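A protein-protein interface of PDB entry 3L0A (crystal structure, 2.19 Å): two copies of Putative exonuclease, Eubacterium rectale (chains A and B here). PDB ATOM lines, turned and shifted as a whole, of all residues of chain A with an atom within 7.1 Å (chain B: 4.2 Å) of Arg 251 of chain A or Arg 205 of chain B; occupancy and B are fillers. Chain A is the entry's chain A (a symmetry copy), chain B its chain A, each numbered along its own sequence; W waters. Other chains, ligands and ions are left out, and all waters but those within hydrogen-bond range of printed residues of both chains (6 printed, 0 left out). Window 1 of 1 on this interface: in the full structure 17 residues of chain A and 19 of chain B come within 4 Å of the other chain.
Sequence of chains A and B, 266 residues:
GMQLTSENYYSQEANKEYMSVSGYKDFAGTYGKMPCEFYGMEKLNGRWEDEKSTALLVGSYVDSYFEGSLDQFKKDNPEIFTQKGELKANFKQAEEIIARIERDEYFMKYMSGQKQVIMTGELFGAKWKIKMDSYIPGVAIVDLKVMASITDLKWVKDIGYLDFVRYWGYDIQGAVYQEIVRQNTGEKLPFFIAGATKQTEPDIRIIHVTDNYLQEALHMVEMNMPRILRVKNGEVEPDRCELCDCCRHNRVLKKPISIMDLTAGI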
ATOM      1  N   PHE A  38      20.150 -13.808  19.269  1.00  0.00           N
ATOM      2  CA  PHE A  38      20.387 -14.093  17.866  1.00  0.00           C
ATOM      3  C   PHE A  38      20.887 -12.855  17.132  1.00  0.00           C
ATOM      4  O   PHE A  38      21.935 -12.887  16.516  1.00  0.00           O
ATOM      5  CB  PHE A  38      19.066 -14.584  17.279  1.00  0.00           C
ATOM      6  CG  PHE A  38      19.123 -14.916  15.818  1.00  0.00           C
ATOM      7  CD1 PHE A  38      19.904 -15.972  15.361  1.00  0.00           C
ATOM      8  CD2 PHE A  38      18.374 -14.202  14.903  1.00  0.00           C
ATOM      9  CE1 PHE A  38      19.953 -16.272  14.004  1.00  0.00           C
ATOM     10  CE2 PHE A  38      18.423 -14.494  13.558  1.00  0.00           C
ATOM     11  CZ  PHE A  38      19.204 -15.512  13.101  1.00  0.00           C
ATOM     12  N   ARG A 240      15.836 -16.281  19.820  1.00  0.00           N
ATOM     13  CA  ARG A 240      15.373 -15.265  18.881  1.00  0.00           C
ATOM     14  C   ARG A 240      14.157 -14.574  19.446  1.00  0.00           C
ATOM     15  O   ARG A 240      13.217 -15.244  19.846  1.00  0.00           O
ATOM     16  CB  ARG A 240      14.967 -15.937  17.579  1.00  0.00           C
ATOM     17  CG  ARG A 240      16.072 -16.699  16.897  1.00  0.00           C
ATOM     18  CD  ARG A 240      15.667 -17.093  15.487  1.00  0.00           C
ATOM     19  NE  ARG A 240      16.712 -17.864  14.798  1.00  0.00           N
ATOM     20  CZ  ARG A 240      16.679 -18.185  13.506  1.00  0.00           C
ATOM     21  NH1 ARG A 240      15.657 -17.831  12.739  1.00  0.00           N
ATOM     22  NH2 ARG A 240      17.662 -18.891  12.968  1.00  0.00           N
ATOM     23  N   CYS A 241      14.154 -13.235  19.464  1.00  0.00           N
ATOM     24  CA  CYS A 241      13.004 -12.499  19.964  1.00  0.00           C
ATOM     25  C   CYS A 241      11.866 -12.679  18.997  1.00  0.00           C
ATOM     26  O   CYS A 241      10.709 -12.556  19.373  1.00  0.00           O
ATOM     27  CB  CYS A 241      13.308 -11.010  20.142  1.00  0.00           C
ATOM     28  SG  CYS A 241      13.542 -10.055  18.603  1.00  0.00           S
ATOM     29  N   GLU A 242      12.196 -12.956  17.744  1.00  0.00           N
ATOM     30  CA  GLU A 242      11.207 -13.082  16.687  1.00  0.00           C
ATOM     31  C   GLU A 242      10.401 -11.785  16.468  1.00  0.00           C
ATOM     32  O   GLU A 242       9.357 -11.814  15.836  1.00  0.00           O
ATOM     33  CB  GLU A 242      10.268 -14.288  16.914  1.00  0.00           C
ATOM     34  CG  GLU A 242      10.954 -15.667  16.971  1.00  0.00           C
ATOM     35  CD  GLU A 242      11.420 -16.192  15.587  1.00  0.00           C
ATOM     36  OE1 GLU A 242      11.309 -15.498  14.547  1.00  0.00           O
ATOM     37  OE2 GLU A 242      11.912 -17.323  15.542  1.00  0.00           O
ATOM     38  N   LEU A 243      10.909 -10.659  16.945  1.00  0.00           N
ATOM     39  CA  LEU A 243      10.243  -9.386  16.767  1.00  0.00           C
ATOM     40  C   LEU A 243      11.126  -8.293  16.132  1.00  0.00           C
ATOM     41  O   LEU A 243      10.709  -7.143  16.062  1.00  0.00           O
ATOM     42  CB  LEU A 243       9.702  -8.895  18.136  1.00  0.00           C
ATOM     43  CG  LEU A 243       8.573  -9.755  18.755  1.00  0.00           C
ATOM     44  CD1 LEU A 243       8.162  -9.236  20.169  1.00  0.00           C
ATOM     45  CD2 LEU A 243       7.337  -9.793  17.830  1.00  0.00           C
ATOM     46  N   CYS A 244      12.337  -8.633  15.684  1.00  0.00           N
ATOM     47  CA  CYS A 244      13.245  -7.663  15.092  1.00  0.00           C
ATOM     48  C   CYS A 244      13.424  -8.019  13.612  1.00  0.00           C
ATOM     49  O   CYS A 244      13.004  -9.090  13.145  1.00  0.00           O
ATOM     50  CB  CYS A 244      14.596  -7.676  15.842  1.00  0.00           C
ATOM     51  SG  CYS A 244      15.513  -9.235  15.634  1.00  0.00           S
ATOM     52  N   ASP A 245      14.037  -7.123  12.861  1.00  0.00           N
ATOM     53  CA  ASP A 245      14.182  -7.283  11.422  1.00  0.00           C
ATOM     54  C   ASP A 245      15.096  -8.481  11.089  1.00  0.00           C
ATOM     55  O   ASP A 245      14.820  -9.248  10.137  1.00  0.00           O
ATOM     56  CB  ASP A 245      14.707  -5.980  10.780  1.00  0.00           C
ATOM     57  CG  ASP A 245      13.611  -4.872  10.604  1.00  0.00           C
ATOM     58  OD1 ASP A 245      12.398  -5.169  10.420  1.00  0.00           O
ATOM     59  OD2 ASP A 245      13.996  -3.674  10.574  1.00  0.00           O
ATOM     60  N   CYS A 246      16.154  -8.656  11.885  1.00  0.00           N
ATOM     61  CA  CYS A 246      17.092  -9.804  11.729  1.00  0.00           C
ATOM     62  C   CYS A 246      16.346 -11.117  11.870  1.00  0.00           C
ATOM     63  O   CYS A 246      16.434 -11.984  11.017  1.00  0.00           O
ATOM     64  CB  CYS A 246      18.244  -9.752  12.764  1.00  0.00           C
ATOM     65  SG  CYS A 246      19.431 -11.101  12.680  1.00  0.00           S
ATOM     66  N   CYS A 247      15.581 -11.227  12.952  1.00  0.00           N
ATOM     67  CA  CYS A 247      14.726 -12.388  13.160  1.00  0.00           C
ATOM     68  C   CYS A 247      13.816 -12.658  11.966  1.00  0.00           C
ATOM     69  O   CYS A 247      13.669 -13.794  11.537  1.00  0.00           O
ATOM     70  CB  CYS A 247      13.908 -12.232  14.445  1.00  0.00           C
ATOM     71  SG  CYS A 247      14.733 -12.877  15.916  1.00  0.00           S
ATOM     72  N   ARG A 248      13.225 -11.607  11.416  1.00  0.00           N
ATOM     73  CA  ARG A 248      12.256 -11.765  10.343  1.00  0.00           C
ATOM     74  C   ARG A 248      12.914 -12.157   9.029  1.00  0.00           C
ATOM     75  O   ARG A 248      12.378 -12.975   8.285  1.00  0.00           O
ATOM     76  CB  ARG A 248      11.418 -10.494  10.158  1.00  0.00           C
ATOM     77  CG  ARG A 248      10.536 -10.129  11.380  1.00  0.00           C
ATOM     78  CD  ARG A 248       9.455  -9.137  11.048  1.00  0.00           C
ATOM     79  NE  ARG A 248       9.948  -7.782  11.192  1.00  0.00           N
ATOM     80  CZ  ARG A 248      10.030  -7.130  12.336  1.00  0.00           C
ATOM     81  NH1 ARG A 248       9.635  -7.661  13.478  1.00  0.00           N
ATOM     82  NH2 ARG A 248      10.522  -5.918  12.336  1.00  0.00           N
ATOM     83  N   HIS A 249      14.055 -11.549   8.735  1.00  0.00           N
ATOM     84  CA  HIS A 249      14.861 -11.919   7.561  1.00  0.00           C
ATOM     85  C   HIS A 249      15.258 -13.374   7.567  1.00  0.00           C
ATOM     86  O   HIS A 249      15.286 -14.019   6.541  1.00  0.00           O
ATOM     87  CB  HIS A 249      16.145 -11.092   7.502  1.00  0.00           C
ATOM     88  CG  HIS A 249      16.981 -11.393   6.300  1.00  0.00           C
ATOM     89  ND1 HIS A 249      16.781 -10.773   5.085  1.00  0.00           N
ATOM     90  CD2 HIS A 249      17.992 -12.276   6.113  1.00  0.00           C
ATOM     91  CE1 HIS A 249      17.658 -11.235   4.211  1.00  0.00           C
ATOM     92  NE2 HIS A 249      18.398 -12.158   4.804  1.00  0.00           N
ATOM     93  N   ASN A 250      15.586 -13.875   8.751  1.00  0.00           N
ATOM     94  CA  ASN A 250      16.080 -15.244   8.910  1.00  0.00           C
ATOM     95  C   ASN A 250      15.036 -16.338   9.165  1.00  0.00           C
ATOM     96  O   ASN A 250      15.389 -17.493   9.264  1.00  0.00           O
ATOM     97  CB  ASN A 250      17.120 -15.231  10.033  1.00  0.00           C
ATOM     98  CG  ASN A 250      18.421 -14.617   9.596  1.00  0.00           C
ATOM     99  OD1 ASN A 250      19.247 -15.299   9.008  1.00  0.00           O
ATOM    100  ND2 ASN A 250      18.625 -13.330   9.891  1.00  0.00           N
ATOM    101  N   ARG A 251      13.748 -15.986   9.265  1.00  0.00           N
ATOM    102  CA  ARG A 251      12.736 -16.967   9.600  1.00  0.00           C
ATOM    103  C   ARG A 251      12.480 -17.880   8.442  1.00  0.00           C
ATOM    104  O   ARG A 251      12.440 -17.424   7.310  1.00  0.00           O
ATOM    105  CB  ARG A 251      11.426 -16.290  10.010  1.00  0.00           C
ATOM    106  CG  ARG A 251      10.352 -17.267  10.450  1.00  0.00           C
ATOM    107  CD  ARG A 251       9.148 -16.573  11.040  1.00  0.00           C
ATOM    108  NE  ARG A 251       9.539 -15.507  11.957  1.00  0.00           N
ATOM    109  CZ  ARG A 251       8.811 -14.425  12.215  1.00  0.00           C
ATOM    110  NH1 ARG A 251       7.637 -14.262  11.643  1.00  0.00           N
ATOM    111  NH2 ARG A 251       9.265 -13.502  13.049  1.00  0.00           N
ATOM    112  N   VAL A 252      12.281 -19.169   8.740  1.00  0.00           N
ATOM    113  CA  VAL A 252      11.995 -20.195   7.759  1.00  0.00           C
ATOM    114  C   VAL A 252      10.844 -20.943   8.347  1.00  0.00           C
ATOM    115  O   VAL A 252      11.006 -21.669   9.328  1.00  0.00           O
ATOM    116  CB  VAL A 252      13.190 -21.149   7.552  1.00  0.00           C
ATOM    117  CG1 VAL A 252      12.851 -22.245   6.544  1.00  0.00           C
ATOM    118  CG2 VAL A 252      14.448 -20.381   7.094  1.00  0.00           C
ATOM    119  N   LEU A 253       9.664 -20.765   7.772  1.00  0.00           N
ATOM    120  CA  LEU A 253       8.453 -21.356   8.322  1.00  0.00           C
ATOM    121  C   LEU A 253       8.350 -22.872   8.086  1.00  0.00           C
ATOM    122  O   LEU A 253       8.685 -23.373   7.008  1.00  0.00           O
ATOM    123  CB  LEU A 253       7.227 -20.708   7.700  1.00  0.00           C
ATOM    124  CG  LEU A 253       7.060 -19.200   7.849  1.00  0.00           C
ATOM    125  CD1 LEU A 253       5.808 -18.891   7.032  1.00  0.00           C
ATOM    126  CD2 LEU A 253       6.899 -18.775   9.302  1.00  0.00           C
ATOM    127  N   LYS A 254       7.862 -23.580   9.099  1.00  0.00           N
ATOM    128  CA  LYS A 254       7.691 -25.006   9.028  1.00  0.00           C
ATOM    129  C   LYS A 254       6.327 -25.408   9.574  1.00  0.00           C
ATOM    130  O   LYS A 254       5.869 -26.528   9.333  1.00  0.00           O
ATOM    131  CB  LYS A 254       8.838 -25.712   9.776  1.00  0.00           C
ATOM    132  CG  LYS A 254       9.921 -26.339   8.842  1.00  0.00           C
ATOM    133  N   LYS A 255       5.640 -24.484  10.267  1.00  0.00           N
ATOM    134  CA  LYS A 255       4.366 -24.826  10.884  1.00  0.00           C
ATOM    135  C   LYS A 255       3.453 -23.633  11.032  1.00  0.00           C
ATOM    136  O   LYS A 255       3.920 -22.495  11.092  1.00  0.00           O
ATOM    137  CB  LYS A 255       4.603 -25.542  12.233  1.00  0.00           C
ATOM    138  CG  LYS A 255       5.580 -24.808  13.199  1.00  0.00           C
ATOM    139  CD  LYS A 255       6.283 -25.810  14.185  1.00  0.00           C
ATOM    140  CE  LYS A 255       7.573 -26.551  13.648  1.00  0.00           C
ATOM    141  NZ  LYS A 255       7.410 -28.030  13.361  1.00  0.00           N
ATOM    142  N   PRO A 256       2.151 -23.878  11.039  1.00  0.00           N
ATOM    143  CA  PRO A 256       1.171 -22.827  11.246  1.00  0.00           C
ATOM    144  C   PRO A 256       1.131 -22.358  12.676  1.00  0.00           C
ATOM    145  O   PRO A 256       1.206 -23.195  13.561  1.00  0.00           O
ATOM    146  CB  PRO A 256      -0.157 -23.512  10.916  1.00  0.00           C
ATOM    147  CG  PRO A 256       0.067 -24.946  11.029  1.00  0.00           C
ATOM    148  CD  PRO A 256       1.527 -25.196  10.835  1.00  0.00           C
ATOM    149  N   ILE A 257       1.050 -21.039  12.914  1.00  0.00           N
ATOM    150  CA  ILE A 257       0.580 -20.552  14.198  1.00  0.00           C
ATOM    151  C   ILE A 257      -0.950 -20.458  14.235  1.00  0.00           C
ATOM    152  O   ILE A 257      -1.634 -20.834  13.275  1.00  0.00           O
ATOM    153  CB  ILE A 257       1.282 -19.213  14.660  1.00  0.00           C
ATOM    154  CG1 ILE A 257       1.001 -18.037  13.739  1.00  0.00           C
ATOM    155  CG2 ILE A 257       2.761 -19.403  14.822  1.00  0.00           C
ATOM    156  CD1 ILE A 257       1.571 -16.686  14.300  1.00  0.00           C
ATOM    157  N   LEU A 262      -0.720 -15.611  19.020  1.00  0.00           N
ATOM    158  CA  LEU A 262      -0.756 -14.131  19.034  1.00  0.00           C
ATOM    159  C   LEU A 262      -1.070 -13.548  20.418  1.00  0.00           C
ATOM    160  O   LEU A 262      -0.587 -12.463  20.723  1.00  0.00           O
ATOM    161  CB  LEU A 262      -1.775 -13.586  18.013  1.00  0.00           C
ATOM    162  CG  LEU A 262      -1.635 -14.161  16.599  1.00  0.00           C
ATOM    163  CD1 LEU A 262      -2.887 -13.918  15.790  1.00  0.00           C
ATOM    164  CD2 LEU A 262      -0.378 -13.597  15.954  1.00  0.00           C
ATOM    165  N   ARG B 100       9.829 -11.890  -0.805  1.00  0.00           N
ATOM    166  CA  ARG B 100      10.051 -12.447   0.519  1.00  0.00           C
ATOM    167  C   ARG B 100       9.231 -13.723   0.755  1.00  0.00           C
ATOM    168  O   ARG B 100       9.761 -14.733   1.262  1.00  0.00           O
ATOM    169  CB  ARG B 100       9.786 -11.404   1.597  1.00  0.00           C
ATOM    170  CG  ARG B 100       9.916 -11.964   3.011  1.00  0.00           C
ATOM    171  CD  ARG B 100      11.305 -12.520   3.220  1.00  0.00           C
ATOM    172  NE  ARG B 100      11.531 -13.066   4.542  1.00  0.00           N
ATOM    173  CZ  ARG B 100      11.620 -14.366   4.847  1.00  0.00           C
ATOM    174  NH1 ARG B 100      11.443 -15.346   3.963  1.00  0.00           N
ATOM    175  NH2 ARG B 100      11.869 -14.697   6.082  1.00  0.00           N
ATOM    176  N   PHE B 107       5.351 -21.383   3.022  1.00  0.00           N
ATOM    177  CA  PHE B 107       4.344 -20.373   2.728  1.00  0.00           C
ATOM    178  C   PHE B 107       3.853 -20.607   1.312  1.00  0.00           C
ATOM    179  O   PHE B 107       2.646 -20.663   1.077  1.00  0.00           O
ATOM    180  CB  PHE B 107       4.945 -18.976   2.902  1.00  0.00           C
ATOM    181  CG  PHE B 107       3.920 -17.797   2.919  1.00  0.00           C
ATOM    182  CD1 PHE B 107       3.123 -17.496   1.820  1.00  0.00           C
ATOM    183  CD2 PHE B 107       3.823 -16.968   4.038  1.00  0.00           C
ATOM    184  CE1 PHE B 107       2.244 -16.413   1.836  1.00  0.00           C
ATOM    185  CE2 PHE B 107       2.957 -15.872   4.063  1.00  0.00           C
ATOM    186  CZ  PHE B 107       2.178 -15.597   2.971  1.00  0.00           C
ATOM    187  N   ILE B 150       1.241  -8.336  12.121  1.00  0.00           N
ATOM    188  CA  ILE B 150       0.651  -9.586  12.573  1.00  0.00           C
ATOM    189  C   ILE B 150       0.570  -9.683  14.103  1.00  0.00           C
ATOM    190  O   ILE B 150      -0.417 -10.151  14.647  1.00  0.00           O
ATOM    191  CB  ILE B 150       1.512 -10.783  12.070  1.00  0.00           C
ATOM    192  CG1 ILE B 150       1.371 -10.947  10.541  1.00  0.00           C
ATOM    193  CG2 ILE B 150       1.156 -12.028  12.807  1.00  0.00           C
ATOM    194  CD1 ILE B 150       2.400 -11.901   9.910  1.00  0.00           C
ATOM    195  N   ILE B 193      -4.938 -17.820   7.231  1.00  0.00           N
ATOM    196  CA  ILE B 193      -4.505 -16.530   6.717  1.00  0.00           C
ATOM    197  C   ILE B 193      -3.021 -16.594   6.453  1.00  0.00           C
ATOM    198  O   ILE B 193      -2.229 -17.007   7.315  1.00  0.00           O
ATOM    199  CB  ILE B 193      -4.822 -15.409   7.718  1.00  0.00           C
ATOM    200  CG1 ILE B 193      -6.346 -15.189   7.763  1.00  0.00           C
ATOM    201  CG2 ILE B 193      -4.096 -14.118   7.333  1.00  0.00           C
ATOM    202  CD1 ILE B 193      -6.851 -14.443   8.993  1.00  0.00           C
ATOM    203  N   ALA B 194      -2.631 -16.254   5.233  1.00  0.00           N
ATOM    204  CA  ALA B 194      -1.224 -16.234   4.876  1.00  0.00           C
ATOM    205  C   ALA B 194      -0.830 -14.769   4.979  1.00  0.00           C
ATOM    206  O   ALA B 194      -1.052 -13.995   4.047  1.00  0.00           O
ATOM    207  CB  ALA B 194      -1.011 -16.790   3.444  1.00  0.00           C
ATOM    208  N   GLY B 195      -0.296 -14.370   6.128  1.00  0.00           N
ATOM    209  CA  GLY B 195       0.006 -12.981   6.377  1.00  0.00           C
ATOM    210  C   GLY B 195       1.432 -12.549   6.072  1.00  0.00           C
ATOM    211  O   GLY B 195       2.405 -13.281   6.394  1.00  0.00           O
ATOM    212  N   ASP B 203       7.407  -9.456   8.178  1.00  0.00           N
ATOM    213  CA  ASP B 203       7.049 -10.592   9.021  1.00  0.00           C
ATOM    214  C   ASP B 203       6.186 -11.506   8.185  1.00  0.00           C
ATOM    215  O   ASP B 203       5.217 -11.040   7.629  1.00  0.00           O
ATOM    216  CB  ASP B 203       6.213 -10.061  10.195  1.00  0.00           C
ATOM    217  CG  ASP B 203       6.199 -10.975  11.403  1.00  0.00           C
ATOM    218  OD1 ASP B 203       7.031 -11.867  11.507  1.00  0.00           O
ATOM    219  OD2 ASP B 203       5.339 -10.763  12.278  1.00  0.00           O
ATOM    220  N   ILE B 204       6.509 -12.787   8.094  1.00  0.00           N
ATOM    221  CA  ILE B 204       5.635 -13.761   7.432  1.00  0.00           C
ATOM    222  C   ILE B 204       5.190 -14.885   8.383  1.00  0.00           C
ATOM    223  O   ILE B 204       6.040 -15.421   9.136  1.00  0.00           O
ATOM    224  CB  ILE B 204       6.293 -14.450   6.163  1.00  0.00           C
ATOM    225  CG1 ILE B 204       7.372 -15.473   6.570  1.00  0.00           C
ATOM    226  CG2 ILE B 204       6.803 -13.401   5.157  1.00  0.00           C
ATOM    227  CD1 ILE B 204       8.249 -15.973   5.452  1.00  0.00           C
ATOM    228  N   ARG B 205       3.893 -15.258   8.288  1.00  0.00           N
ATOM    229  CA  ARG B 205       3.257 -16.330   9.070  1.00  0.00           C
ATOM    230  C   ARG B 205       2.103 -16.951   8.306  1.00  0.00           C
ATOM    231  O   ARG B 205       1.350 -16.241   7.644  1.00  0.00           O
ATOM    232  CB  ARG B 205       2.614 -15.784  10.363  1.00  0.00           C
ATOM    233  CG  ARG B 205       3.523 -15.274  11.442  1.00  0.00           C
ATOM    234  CD  ARG B 205       4.448 -16.296  11.962  1.00  0.00           C
ATOM    235  NE  ARG B 205       5.298 -15.751  13.025  1.00  0.00           N
ATOM    236  CZ  ARG B 205       6.166 -16.494  13.722  1.00  0.00           C
ATOM    237  NH1 ARG B 205       6.304 -17.795  13.470  1.00  0.00           N
ATOM    238  NH2 ARG B 205       6.899 -15.944  14.681  1.00  0.00           N
ATOM    239  N   ILE B 206       1.925 -18.257   8.465  1.00  0.00           N
ATOM    240  CA  ILE B 206       0.664 -18.947   8.176  1.00  0.00           C
ATOM    241  C   ILE B 206      -0.117 -19.065   9.484  1.00  0.00           C
ATOM    242  O   ILE B 206       0.388 -19.630  10.450  1.00  0.00           O
ATOM    243  CB  ILE B 206       0.926 -20.359   7.598  1.00  0.00           C
ATOM    244  CG1 ILE B 206       1.558 -20.274   6.204  1.00  0.00           C
ATOM    245  CG2 ILE B 206      -0.365 -21.129   7.453  1.00  0.00           C
ATOM    246  CD1 ILE B 206       0.747 -19.332   5.169  1.00  0.00           C
ATOM    247  N   ILE B 207      -1.329 -18.509   9.556  1.00  0.00           N
ATOM    248  CA  ILE B 207      -2.111 -18.539  10.794  1.00  0.00           C
ATOM    249  C   ILE B 207      -3.403 -19.352  10.612  1.00  0.00           C
ATOM    250  O   ILE B 207      -4.283 -18.949   9.850  1.00  0.00           O
ATOM    251  CB  ILE B 207      -2.484 -17.144  11.237  1.00  0.00           C
ATOM    252  CG1 ILE B 207      -1.238 -16.269  11.336  1.00  0.00           C
ATOM    253  CG2 ILE B 207      -3.238 -17.166  12.601  1.00  0.00           C
ATOM    254  CD1 ILE B 207      -1.369 -14.932  10.728  1.00  0.00           C
HETATM  255  O   HOH W   1       3.499 -19.907  10.426  1.00  0.00           O
HETATM  256  O   HOH W   2       8.170 -10.104  13.939  1.00  0.00           O
HETATM  257  O   HOH W   3      11.613 -18.020   4.859  1.00  0.00           O
HETATM  258  O   HOH W   4      11.991 -10.798   6.384  1.00  0.00           O
HETATM  259  O   HOH W   5       9.708 -12.761   8.677  1.00  0.00           O
HETATM  260  O   HOH W   6       5.733 -20.181  12.461  1.00  0.00           O
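NH2 of Arg 100 of chain B is in hydrogen-bond range of O of Arg 248 of chain A (2.8 Å).
NH2 of Arg 100 of chain B is in hydrogen-bond range of O of Arg 251 of chain A.
NH1 of Arg 251 of chain A is in salt-bridge range of OD1 of Asp 203 of chain B.
NH1 of Arg 251 of chain A sits at hydrogen-bond distance from O of Ile 204 of chain B (3.2 Å).
N of Ile 257 of chain A is in hydrogen-bond range of O of Ile 206 of chain B (2.9 Å).
The guanidinium group (NE) of Arg 205 of chain B sits close to the guanidinium group (NH1) of Arg 251 of chain A, at 3.1 Å.
The backbone carbonyl oxygen (O) of Ile 193 of chain B sits at hydrogen-bond distance from the backbone NH (N) of Ile 207 of chain B (2.8 Å).
The backbone NH (N) of Gly 195 of chain B is in hydrogen-bond range of the backbone carbonyl oxygen (O) of Arg 205 of chain B, 2.9 Å away.
The side-chain carboxylate (OE1) of Glu 242 of chain A lies within salt-bridge range of the guanidinium group (NE) of Arg 251 of chain A.
The backbone carbonyl oxygen (O) of Leu 243 of chain A is in hydrogen-bond range of the guanidinium group (NH1) of Arg 248 of chain A (2.8 Å).
OD1 of Asp 245 of chain A is in salt-bridge range of NH2 of Arg 248 of chain A.
Among the printed residues, pairs that only touch across the chains: Pro 256 of chain A with Ile 206 of chain B (3.4 Å), Ile 257 of chain A with Ile 207 of chain B (3.4 Å), Arg 248 of chain A with Asp 203 of chain B (3.5 Å), Leu 253 of chain A with Ile 204 of chain B (3.5 Å), His 249 of chain A with Arg 100 of chain B (3.5 Å), Leu 262 of chain A with Ile 150 of chain B (3.7 Å) and Ile 257 of chain A with Arg 205 of chain B (3.7 Å).
Leu 243 of chain A touches none of the printed residues of chain B.
Of the printed residues of chain B, Arg 251 of chain A touches Arg 100 (3.0 Å), Asp 203 (2.5 Å), Ile 204 (3.2 Å) and Arg 205 (3.1 Å).
Of the printed residues of chain B, Leu 253 of chain A touches Ile 204 (3.5 Å).
Of the printed residues of chain B, Ile 257 of chain A touches Arg 205, Ile 206 and Ile 207.
Printed residues of chain A within 4 Å of Arg 100 of chain B: Arg 248, His 249 and Arg 251.
Of chain A, only Arg 251 and Ile 257 come within 4 Å of Arg 205 of chain B.
The nearest printed residue of chain B that does not touch Arg 251 of chain A is Ile 150 of chain B (6.0 Å).
Hydrophobic or aromatic side chains of chain A within 4 Å of the printed part of chain B: Leu 253, Pro 256, Ile 257 and Leu 262.
Of the 11 printed residues of chain B, 7 touch a printed residue of chain A.
Printed residues of chain B that touch a printed residue of chain A: Arg 100, Ile 150, Asp 203, Ile 204, Arg 205, Ile 206 and Ile 207.
Among the printed residues, 13 pairs touch across the chains.
Among the printed residues, Asp or Glu carboxylates within 4 Å of a Lys or Arg side-chain nitrogen of the other chain: Arg 251 of chain A with Asp 203 of chain B.
No position is printed for both chains.
Of the 13 pairs that touch across the chains among the printed residues, none has its exchanged pair printed and touching as well.
Water W6 lies within hydrogen-bond range of the guanidinium group of Arg 205 of chain B (2.7 Å) and the backbone carbonyl oxygen of Lys 255 of chain A (3.2 Å).
Water W3 bridges O of Arg 251 of chain A and NH1 of Arg 100 of chain B.
Water W1 bridges O of Lys 255 of chain A and N of Ile 206 of chain B.
Water W5 bridges the backbone carbonyl oxygen (O) of Arg 248 of chain A (2.7 Å) and the backbone NH (N) of Ile 204 of chain B (3.3 Å).
Water W2 lies within hydrogen-bond range of O of Glu 242 of chain A (2.8 Å), NH1 of Arg 248 of chain A (2.9 Å) and OD1 of Asp 203 of chain B (3.2 Å).
Water W4 lies within hydrogen-bond range of the backbone carbonyl oxygen of Arg 248 of chain A (2.9 Å), the guanidinium group of Arg 100 of chain B (3.0 Å) and the backbone NH of His 249 of chain A (3.2 Å).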
